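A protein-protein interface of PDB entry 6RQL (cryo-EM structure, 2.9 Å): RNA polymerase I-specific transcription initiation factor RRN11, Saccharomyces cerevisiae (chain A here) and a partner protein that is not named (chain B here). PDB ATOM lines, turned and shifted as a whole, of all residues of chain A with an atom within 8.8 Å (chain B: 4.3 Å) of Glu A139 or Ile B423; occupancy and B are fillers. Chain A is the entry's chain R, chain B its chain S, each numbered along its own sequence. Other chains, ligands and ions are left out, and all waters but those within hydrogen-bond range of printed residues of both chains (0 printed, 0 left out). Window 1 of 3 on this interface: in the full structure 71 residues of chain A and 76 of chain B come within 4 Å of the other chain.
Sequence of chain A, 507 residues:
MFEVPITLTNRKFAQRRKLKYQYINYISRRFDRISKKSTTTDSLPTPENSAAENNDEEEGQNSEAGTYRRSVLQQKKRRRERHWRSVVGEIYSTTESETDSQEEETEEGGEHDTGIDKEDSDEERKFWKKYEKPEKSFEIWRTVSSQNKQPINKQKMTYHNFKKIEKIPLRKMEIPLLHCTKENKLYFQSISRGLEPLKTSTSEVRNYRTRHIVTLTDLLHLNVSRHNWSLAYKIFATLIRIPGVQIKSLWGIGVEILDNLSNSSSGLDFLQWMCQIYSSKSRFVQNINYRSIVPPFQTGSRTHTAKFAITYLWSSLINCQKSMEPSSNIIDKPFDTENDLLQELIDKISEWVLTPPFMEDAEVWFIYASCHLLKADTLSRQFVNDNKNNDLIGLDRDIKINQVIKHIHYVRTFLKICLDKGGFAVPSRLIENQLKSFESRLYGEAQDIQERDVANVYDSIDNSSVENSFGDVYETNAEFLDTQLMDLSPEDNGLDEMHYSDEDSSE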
ATOM      1  N   GLU A 132      11.819 -13.447 -26.276  1.00  0.00           N
ATOM      2  CA  GLU A 132      12.829 -14.374 -26.763  1.00  0.00           C
ATOM      3  C   GLU A 132      14.128 -14.135 -26.009  1.00  0.00           C
ATOM      4  O   GLU A 132      14.737 -13.070 -26.138  1.00  0.00           O
ATOM      5  CB  GLU A 132      13.046 -14.195 -28.262  1.00  0.00           C
ATOM      6  CG  GLU A 132      11.842 -14.539 -29.125  1.00  0.00           C
ATOM      7  CD  GLU A 132      11.555 -16.023 -29.161  1.00  0.00           C
ATOM      8  OE1 GLU A 132      12.516 -16.813 -29.050  1.00  0.00           O
ATOM      9  OE2 GLU A 132      10.375 -16.399 -29.320  1.00  0.00           O
ATOM     10  N   LYS A 133      14.537 -15.117 -25.227  1.00  0.00           N
ATOM     11  CA  LYS A 133      15.832 -15.109 -24.562  1.00  0.00           C
ATOM     12  C   LYS A 133      16.931 -15.328 -25.596  1.00  0.00           C
ATOM     13  O   LYS A 133      16.857 -16.286 -26.369  1.00  0.00           O
ATOM     14  CB  LYS A 133      15.862 -16.201 -23.504  1.00  0.00           C
ATOM     15  CG  LYS A 133      14.818 -15.992 -22.431  1.00  0.00           C
ATOM     16  CD  LYS A 133      14.749 -17.134 -21.448  1.00  0.00           C
ATOM     17  CE  LYS A 133      13.577 -16.931 -20.505  1.00  0.00           C
ATOM     18  NZ  LYS A 133      13.383 -18.040 -19.537  1.00  0.00           N
ATOM     19  N   PRO A 134      17.950 -14.466 -25.648  1.00  0.00           N
ATOM     20  CA  PRO A 134      18.823 -14.423 -26.827  1.00  0.00           C
ATOM     21  C   PRO A 134      19.768 -15.601 -26.992  1.00  0.00           C
ATOM     22  O   PRO A 134      20.010 -16.017 -28.131  1.00  0.00           O
ATOM     23  CB  PRO A 134      19.613 -13.127 -26.619  1.00  0.00           C
ATOM     24  CG  PRO A 134      18.814 -12.338 -25.680  1.00  0.00           C
ATOM     25  CD  PRO A 134      18.187 -13.317 -24.772  1.00  0.00           C
ATOM     26  N   GLU A 135      20.411 -16.035 -25.902  1.00  0.00           N
ATOM     27  CA  GLU A 135      21.176 -17.278 -25.785  1.00  0.00           C
ATOM     28  C   GLU A 135      22.489 -17.264 -26.576  1.00  0.00           C
ATOM     29  O   GLU A 135      23.342 -18.135 -26.392  1.00  0.00           O
ATOM     30  CB  GLU A 135      20.272 -18.457 -26.176  1.00  0.00           C
ATOM     31  CG  GLU A 135      20.681 -19.829 -25.735  1.00  0.00           C
ATOM     32  CD  GLU A 135      21.475 -20.545 -26.771  1.00  0.00           C
ATOM     33  OE1 GLU A 135      21.361 -20.166 -27.950  1.00  0.00           O
ATOM     34  OE2 GLU A 135      22.184 -21.507 -26.408  1.00  0.00           O
ATOM     35  N   LYS A 136      22.698 -16.249 -27.409  1.00  0.00           N
ATOM     36  CA  LYS A 136      23.981 -15.935 -28.013  1.00  0.00           C
ATOM     37  C   LYS A 136      24.577 -14.680 -27.416  1.00  0.00           C
ATOM     38  O   LYS A 136      25.797 -14.567 -27.312  1.00  0.00           O
ATOM     39  CB  LYS A 136      23.817 -15.689 -29.521  1.00  0.00           C
ATOM     40  CG  LYS A 136      23.173 -16.790 -30.349  1.00  0.00           C
ATOM     41  CD  LYS A 136      24.087 -17.949 -30.657  1.00  0.00           C
ATOM     42  CE  LYS A 136      25.145 -17.585 -31.682  1.00  0.00           C
ATOM     43  NZ  LYS A 136      25.932 -18.772 -32.110  1.00  0.00           N
ATOM     44  N   SER A 137      23.714 -13.747 -27.024  1.00  0.00           N
ATOM     45  CA  SER A 137      24.076 -12.420 -26.579  1.00  0.00           C
ATOM     46  C   SER A 137      23.340 -12.135 -25.286  1.00  0.00           C
ATOM     47  O   SER A 137      22.374 -12.815 -24.938  1.00  0.00           O
ATOM     48  CB  SER A 137      23.705 -11.378 -27.627  1.00  0.00           C
ATOM     49  OG  SER A 137      22.304 -11.323 -27.789  1.00  0.00           O
ATOM     50  N   PHE A 138      23.787 -11.108 -24.567  1.00  0.00           N
ATOM     51  CA  PHE A 138      23.052 -10.714 -23.375  1.00  0.00           C
ATOM     52  C   PHE A 138      21.745 -10.025 -23.735  1.00  0.00           C
ATOM     53  O   PHE A 138      20.807 -10.024 -22.934  1.00  0.00           O
ATOM     54  CB  PHE A 138      23.907  -9.795 -22.502  1.00  0.00           C
ATOM     55  CG  PHE A 138      25.143 -10.454 -21.955  1.00  0.00           C
ATOM     56  CD1 PHE A 138      25.083 -11.230 -20.811  1.00  0.00           C
ATOM     57  CD2 PHE A 138      26.364 -10.296 -22.589  1.00  0.00           C
ATOM     58  CE1 PHE A 138      26.216 -11.839 -20.309  1.00  0.00           C
ATOM     59  CE2 PHE A 138      27.502 -10.901 -22.089  1.00  0.00           C
ATOM     60  CZ  PHE A 138      27.428 -11.674 -20.949  1.00  0.00           C
ATOM     61  N   GLU A 139      21.683  -9.434 -24.923  1.00  0.00           N
ATOM     62  CA  GLU A 139      20.571  -8.639 -25.411  1.00  0.00           C
ATOM     63  C   GLU A 139      20.283  -9.094 -26.826  1.00  0.00           C
ATOM     64  O   GLU A 139      21.212  -9.248 -27.620  1.00  0.00           O
ATOM     65  CB  GLU A 139      20.956  -7.184 -25.452  1.00  0.00           C
ATOM     66  CG  GLU A 139      21.375  -6.614 -24.147  1.00  0.00           C
ATOM     67  CD  GLU A 139      22.230  -5.398 -24.345  1.00  0.00           C
ATOM     68  OE1 GLU A 139      22.646  -5.151 -25.494  1.00  0.00           O
ATOM     69  OE2 GLU A 139      22.496  -4.693 -23.359  1.00  0.00           O
ATOM     70  N   ILE A 140      19.014  -9.282 -27.170  1.00  0.00           N
ATOM     71  CA  ILE A 140      18.743  -9.711 -28.535  1.00  0.00           C
ATOM     72  C   ILE A 140      18.788  -8.489 -29.453  1.00  0.00           C
ATOM     73  O   ILE A 140      17.791  -7.792 -29.667  1.00  0.00           O
ATOM     74  CB  ILE A 140      17.439 -10.540 -28.621  1.00  0.00           C
ATOM     75  CG1 ILE A 140      17.133 -10.968 -30.056  1.00  0.00           C
ATOM     76  CG2 ILE A 140      16.274  -9.934 -27.846  1.00  0.00           C
ATOM     77  CD1 ILE A 140      16.125 -12.090 -30.142  1.00  0.00           C
ATOM     78  N   TRP A 141      19.984  -8.214 -29.970  1.00  0.00           N
ATOM     79  CA  TRP A 141      20.219  -7.110 -30.888  1.00  0.00           C
ATOM     80  C   TRP A 141      19.517  -7.341 -32.215  1.00  0.00           C
ATOM     81  O   TRP A 141      19.217  -8.473 -32.599  1.00  0.00           O
ATOM     82  CB  TRP A 141      21.708  -6.945 -31.165  1.00  0.00           C
ATOM     83  CG  TRP A 141      22.534  -6.321 -30.104  1.00  0.00           C
ATOM     84  CD1 TRP A 141      23.222  -6.955 -29.120  1.00  0.00           C
ATOM     85  CD2 TRP A 141      22.832  -4.935 -29.971  1.00  0.00           C
ATOM     86  NE1 TRP A 141      23.902  -6.044 -28.356  1.00  0.00           N
ATOM     87  CE2 TRP A 141      23.679  -4.793 -28.864  1.00  0.00           C
ATOM     88  CE3 TRP A 141      22.441  -3.793 -30.665  1.00  0.00           C
ATOM     89  CZ2 TRP A 141      24.152  -3.556 -28.446  1.00  0.00           C
ATOM     90  CZ3 TRP A 141      22.930  -2.568 -30.262  1.00  0.00           C
ATOM     91  CH2 TRP A 141      23.761  -2.458 -29.154  1.00  0.00           C
ATOM     92  N   ARG A 142      19.270  -6.247 -32.931  1.00  0.00           N
ATOM     93  CA  ARG A 142      18.630  -6.281 -34.238  1.00  0.00           C
ATOM     94  C   ARG A 142      19.361  -5.335 -35.173  1.00  0.00           C
ATOM     95  O   ARG A 142      19.851  -4.290 -34.741  1.00  0.00           O
ATOM     96  CB  ARG A 142      17.155  -5.885 -34.133  1.00  0.00           C
ATOM     97  CG  ARG A 142      16.320  -6.901 -33.382  1.00  0.00           C
ATOM     98  CD  ARG A 142      14.929  -6.423 -33.065  1.00  0.00           C
ATOM     99  NE  ARG A 142      14.264  -7.393 -32.209  1.00  0.00           N
ATOM    100  CZ  ARG A 142      13.099  -7.188 -31.608  1.00  0.00           C
ATOM    101  NH1 ARG A 142      12.465  -6.033 -31.757  1.00  0.00           N
ATOM    102  NH2 ARG A 142      12.578  -8.139 -30.845  1.00  0.00           N
ATOM    103  N   PRO A 296      25.154 -16.649 -22.553  1.00  0.00           N
ATOM    104  CA  PRO A 296      26.001 -16.050 -23.600  1.00  0.00           C
ATOM    105  C   PRO A 296      27.496 -16.005 -23.310  1.00  0.00           C
ATOM    106  O   PRO A 296      28.242 -15.523 -24.161  1.00  0.00           O
ATOM    107  CB  PRO A 296      25.460 -14.622 -23.701  1.00  0.00           C
ATOM    108  CG  PRO A 296      24.200 -14.633 -22.983  1.00  0.00           C
ATOM    109  CD  PRO A 296      24.403 -15.569 -21.897  1.00  0.00           C
ATOM    110  N   VAL B 394      17.907  -2.636 -29.492  1.00  0.00           N
ATOM    111  CA  VAL B 394      18.294  -3.464 -28.360  1.00  0.00           C
ATOM    112  C   VAL B 394      17.017  -3.976 -27.723  1.00  0.00           C
ATOM    113  O   VAL B 394      16.004  -3.278 -27.709  1.00  0.00           O
ATOM    114  CB  VAL B 394      19.136  -2.650 -27.355  1.00  0.00           C
ATOM    115  CG1 VAL B 394      19.647  -3.497 -26.197  1.00  0.00           C
ATOM    116  CG2 VAL B 394      20.277  -1.996 -28.043  1.00  0.00           C
ATOM    117  N   GLN B 395      17.041  -5.207 -27.234  1.00  0.00           N
ATOM    118  CA  GLN B 395      16.024  -5.692 -26.311  1.00  0.00           C
ATOM    119  C   GLN B 395      16.738  -6.416 -25.182  1.00  0.00           C
ATOM    120  O   GLN B 395      17.390  -7.440 -25.409  1.00  0.00           O
ATOM    121  CB  GLN B 395      15.032  -6.605 -27.005  1.00  0.00           C
ATOM    122  CG  GLN B 395      13.991  -7.123 -26.075  1.00  0.00           C
ATOM    123  CD  GLN B 395      13.063  -8.066 -26.762  1.00  0.00           C
ATOM    124  OE1 GLN B 395      13.208  -8.336 -27.952  1.00  0.00           O
ATOM    125  NE2 GLN B 395      12.114  -8.598 -26.021  1.00  0.00           N
ATOM    126  N   ALA B 396      16.607  -5.889 -23.970  1.00  0.00           N
ATOM    127  CA  ALA B 396      17.422  -6.302 -22.838  1.00  0.00           C
ATOM    128  C   ALA B 396      16.543  -6.698 -21.669  1.00  0.00           C
ATOM    129  O   ALA B 396      16.628  -6.095 -20.600  1.00  0.00           O
ATOM    130  CB  ALA B 396      18.375  -5.185 -22.417  1.00  0.00           C
ATOM    131  N   SER B 400      20.187  -9.103 -18.996  1.00  0.00           N
ATOM    132  CA  SER B 400      20.817  -7.840 -18.674  1.00  0.00           C
ATOM    133  C   SER B 400      19.745  -6.766 -18.691  1.00  0.00           C
ATOM    134  O   SER B 400      18.558  -7.055 -18.829  1.00  0.00           O
ATOM    135  CB  SER B 400      21.959  -7.509 -19.636  1.00  0.00           C
ATOM    136  OG  SER B 400      21.470  -7.230 -20.927  1.00  0.00           O
ATOM    137  N   ILE B 414      29.387   5.965 -30.265  1.00  0.00           N
ATOM    138  CA  ILE B 414      28.721   6.317 -29.014  1.00  0.00           C
ATOM    139  C   ILE B 414      28.764   5.106 -28.090  1.00  0.00           C
ATOM    140  O   ILE B 414      28.517   3.976 -28.522  1.00  0.00           O
ATOM    141  CB  ILE B 414      27.269   6.787 -29.257  1.00  0.00           C
ATOM    142  CG1 ILE B 414      27.229   8.109 -30.018  1.00  0.00           C
ATOM    143  CG2 ILE B 414      26.546   6.997 -27.971  1.00  0.00           C
ATOM    144  CD1 ILE B 414      25.856   8.496 -30.445  1.00  0.00           C
ATOM    145  N   LEU B 415      29.087   5.336 -26.821  1.00  0.00           N
ATOM    146  CA  LEU B 415      29.253   4.263 -25.858  1.00  0.00           C
ATOM    147  C   LEU B 415      27.965   4.047 -25.069  1.00  0.00           C
ATOM    148  O   LEU B 415      27.342   5.003 -24.602  1.00  0.00           O
ATOM    149  CB  LEU B 415      30.411   4.589 -24.916  1.00  0.00           C
ATOM    150  CG  LEU B 415      31.135   3.410 -24.268  1.00  0.00           C
ATOM    151  CD1 LEU B 415      32.562   3.808 -23.957  1.00  0.00           C
ATOM    152  CD2 LEU B 415      30.455   2.897 -23.029  1.00  0.00           C
ATOM    153  N   LEU B 416      27.594   2.778 -24.899  1.00  0.00           N
ATOM    154  CA  LEU B 416      26.423   2.358 -24.138  1.00  0.00           C
ATOM    155  C   LEU B 416      26.856   1.514 -22.950  1.00  0.00           C
ATOM    156  O   LEU B 416      27.741   0.667 -23.076  1.00  0.00           O
ATOM    157  CB  LEU B 416      25.451   1.550 -25.012  1.00  0.00           C
ATOM    158  CG  LEU B 416      24.251   0.878 -24.336  1.00  0.00           C
ATOM    159  CD1 LEU B 416      23.331   1.884 -23.707  1.00  0.00           C
ATOM    160  CD2 LEU B 416      23.492  -0.001 -25.296  1.00  0.00           C
ATOM    161  N   SER B 418      25.340  -1.188 -20.650  1.00  0.00           N
ATOM    162  CA  SER B 418      24.443  -2.127 -20.028  1.00  0.00           C
ATOM    163  C   SER B 418      25.080  -2.630 -18.744  1.00  0.00           C
ATOM    164  O   SER B 418      26.248  -2.369 -18.460  1.00  0.00           O
ATOM    165  CB  SER B 418      24.154  -3.285 -20.967  1.00  0.00           C
ATOM    166  OG  SER B 418      23.329  -4.242 -20.341  1.00  0.00           O
ATOM    167  N   ILE B 421      28.080  -5.714 -19.490  1.00  0.00           N
ATOM    168  CA  ILE B 421      28.830  -5.465 -20.716  1.00  0.00           C
ATOM    169  C   ILE B 421      28.910  -3.962 -20.963  1.00  0.00           C
ATOM    170  O   ILE B 421      28.014  -3.205 -20.580  1.00  0.00           O
ATOM    171  CB  ILE B 421      28.206  -6.243 -21.906  1.00  0.00           C
ATOM    172  CG1 ILE B 421      29.211  -6.434 -23.032  1.00  0.00           C
ATOM    173  CG2 ILE B 421      26.947  -5.583 -22.425  1.00  0.00           C
ATOM    174  CD1 ILE B 421      28.859  -7.591 -23.917  1.00  0.00           C
ATOM    175  N   ILE B 422      30.026  -3.530 -21.549  1.00  0.00           N
ATOM    176  CA  ILE B 422      30.251  -2.158 -22.003  1.00  0.00           C
ATOM    177  C   ILE B 422      30.250  -2.167 -23.524  1.00  0.00           C
ATOM    178  O   ILE B 422      31.080  -2.840 -24.137  1.00  0.00           O
ATOM    179  CB  ILE B 422      31.576  -1.598 -21.460  1.00  0.00           C
ATOM    180  CG1 ILE B 422      31.460  -1.265 -19.982  1.00  0.00           C
ATOM    181  CG2 ILE B 422      32.026  -0.370 -22.220  1.00  0.00           C
ATOM    182  CD1 ILE B 422      30.498  -0.125 -19.712  1.00  0.00           C
ATOM    183  N   ILE B 423      29.340  -1.415 -24.136  1.00  0.00           N
ATOM    184  CA  ILE B 423      29.142  -1.451 -25.581  1.00  0.00           C
ATOM    185  C   ILE B 423      29.486  -0.087 -26.162  1.00  0.00           C
ATOM    186  O   ILE B 423      29.109   0.947 -25.604  1.00  0.00           O
ATOM    187  CB  ILE B 423      27.698  -1.854 -25.931  1.00  0.00           C
ATOM    188  CG1 ILE B 423      27.360  -3.176 -25.268  1.00  0.00           C
ATOM    189  CG2 ILE B 423      27.526  -2.038 -27.417  1.00  0.00           C
ATOM    190  CD1 ILE B 423      25.910  -3.498 -25.307  1.00  0.00           C
ATOM    191  N   VAL B 424      30.201  -0.088 -27.288  1.00  0.00           N
ATOM    192  CA  VAL B 424      30.723   1.117 -27.925  1.00  0.00           C
ATOM    193  C   VAL B 424      30.037   1.229 -29.287  1.00  0.00           C
ATOM    194  O   VAL B 424      30.687   1.448 -30.313  1.00  0.00           O
ATOM    195  CB  VAL B 424      32.263   1.077 -28.028  1.00  0.00           C
ATOM    196  CG1 VAL B 424      32.870   2.457 -28.305  1.00  0.00           C
ATOM    197  CG2 VAL B 424      32.854   0.526 -26.766  1.00  0.00           C
ATOM    198  N   GLY B 425      28.740   0.942 -29.324  1.00  0.00           N
ATOM    199  CA  GLY B 425      27.974   0.918 -30.559  1.00  0.00           C
ATOM    200  C   GLY B 425      27.961   2.176 -31.410  1.00  0.00           C
ATOM    201  O   GLY B 425      27.350   3.185 -31.056  1.00  0.00           O
ATOM    202  N   LYS B 439      32.576  -4.505 -28.191  1.00  0.00           N
ATOM    203  CA  LYS B 439      32.075  -4.383 -26.834  1.00  0.00           C
ATOM    204  C   LYS B 439      32.813  -5.334 -25.900  1.00  0.00           C
ATOM    205  O   LYS B 439      33.367  -6.348 -26.326  1.00  0.00           O
ATOM    206  CB  LYS B 439      30.573  -4.651 -26.803  1.00  0.00           C
ATOM    207  CG  LYS B 439      30.182  -6.064 -27.078  1.00  0.00           C
ATOM    208  CD  LYS B 439      28.688  -6.207 -27.333  1.00  0.00           C
ATOM    209  CE  LYS B 439      28.317  -5.806 -28.743  1.00  0.00           C
ATOM    210  NZ  LYS B 439      26.921  -6.186 -29.010  1.00  0.00           N
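N of Ile A140 sits at hydrogen-bond distance from O of Gln B395 (3.0 Å). OE1 of Gln B395 sits at hydrogen-bond distance from NH2 of Arg A142 (3.0 Å). The side-chain carboxylate (OE2) of Glu A139 is in hydrogen-bond range of the side-chain hydroxyl (OG) of Ser B418. The indole nitrogen (NE1) of Trp A141 sits close to the side-chain amino group (NZ) of Lys B439, 3.1 Å away.
N of Leu B416 is in hydrogen-bond range of O of Ile B423. The backbone NH (N) of Glu A139 sits close to the side-chain hydroxyl (OG) of Ser A137, 3.5 Å away. The side-chain carboxylate of Glu A139 sits at hydrogen-bond distance from the indole nitrogen of Trp A141, 3.3 Å away.
Among the printed residues, merely in contact across the chains: Phe A138 with Ser B400, Phe A138 with Ile B421, Glu A139 with Val B394, Glu A139 with Gln B395, Glu A139 with Ala B396, Glu A139 with Ser B400, Glu A139 with Ile B423, Trp A141 with Val B394 and Trp A141 with Ile B423.
Printed residues of chain B within 4 Å of Phe A138: Ser B400 and Ile B421. Glu A139 touches just these residues of chain B: Val B394, Gln B395, Ala B396, Ser B400, Ser B418 and Ile B423. Printed residues of chain A within 4 Å of Ile B421: Phe A138. Of chain A, only Glu A139 and Trp A141 come within 4 Å of Ile B423. Of the printed residues of chain A, Lys B439 touches Trp A141 (3.1 Å). The nearest printed residue of chain B that does not touch Glu A139 is Ile B421 (4.6 Å). The nearest residue of chain A that does not touch Ile B423 is Phe A138 (7.2 Å). The nearest printed residue of chain A that does not touch Lys B439 is Glu A139 (5.6 Å).
Of the 14 printed residues of chain B, 8 touch a printed residue of chain A. Printed residues of chain B that touch a printed residue of chain A: Val B394, Gln B395, Ala B396, Ser B400, Ser B418, Ile B421, Ile B423 and Lys B439. Hydrophobic or aromatic side chains of chain B within 4 Å of the printed part of chain A: Val B394, Ala B396, Ile B421 and Ile B423. Hydrophobic or aromatic side chains of chain A that line the printed part of chain B: Phe A138, Ile A140 and Trp A141.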
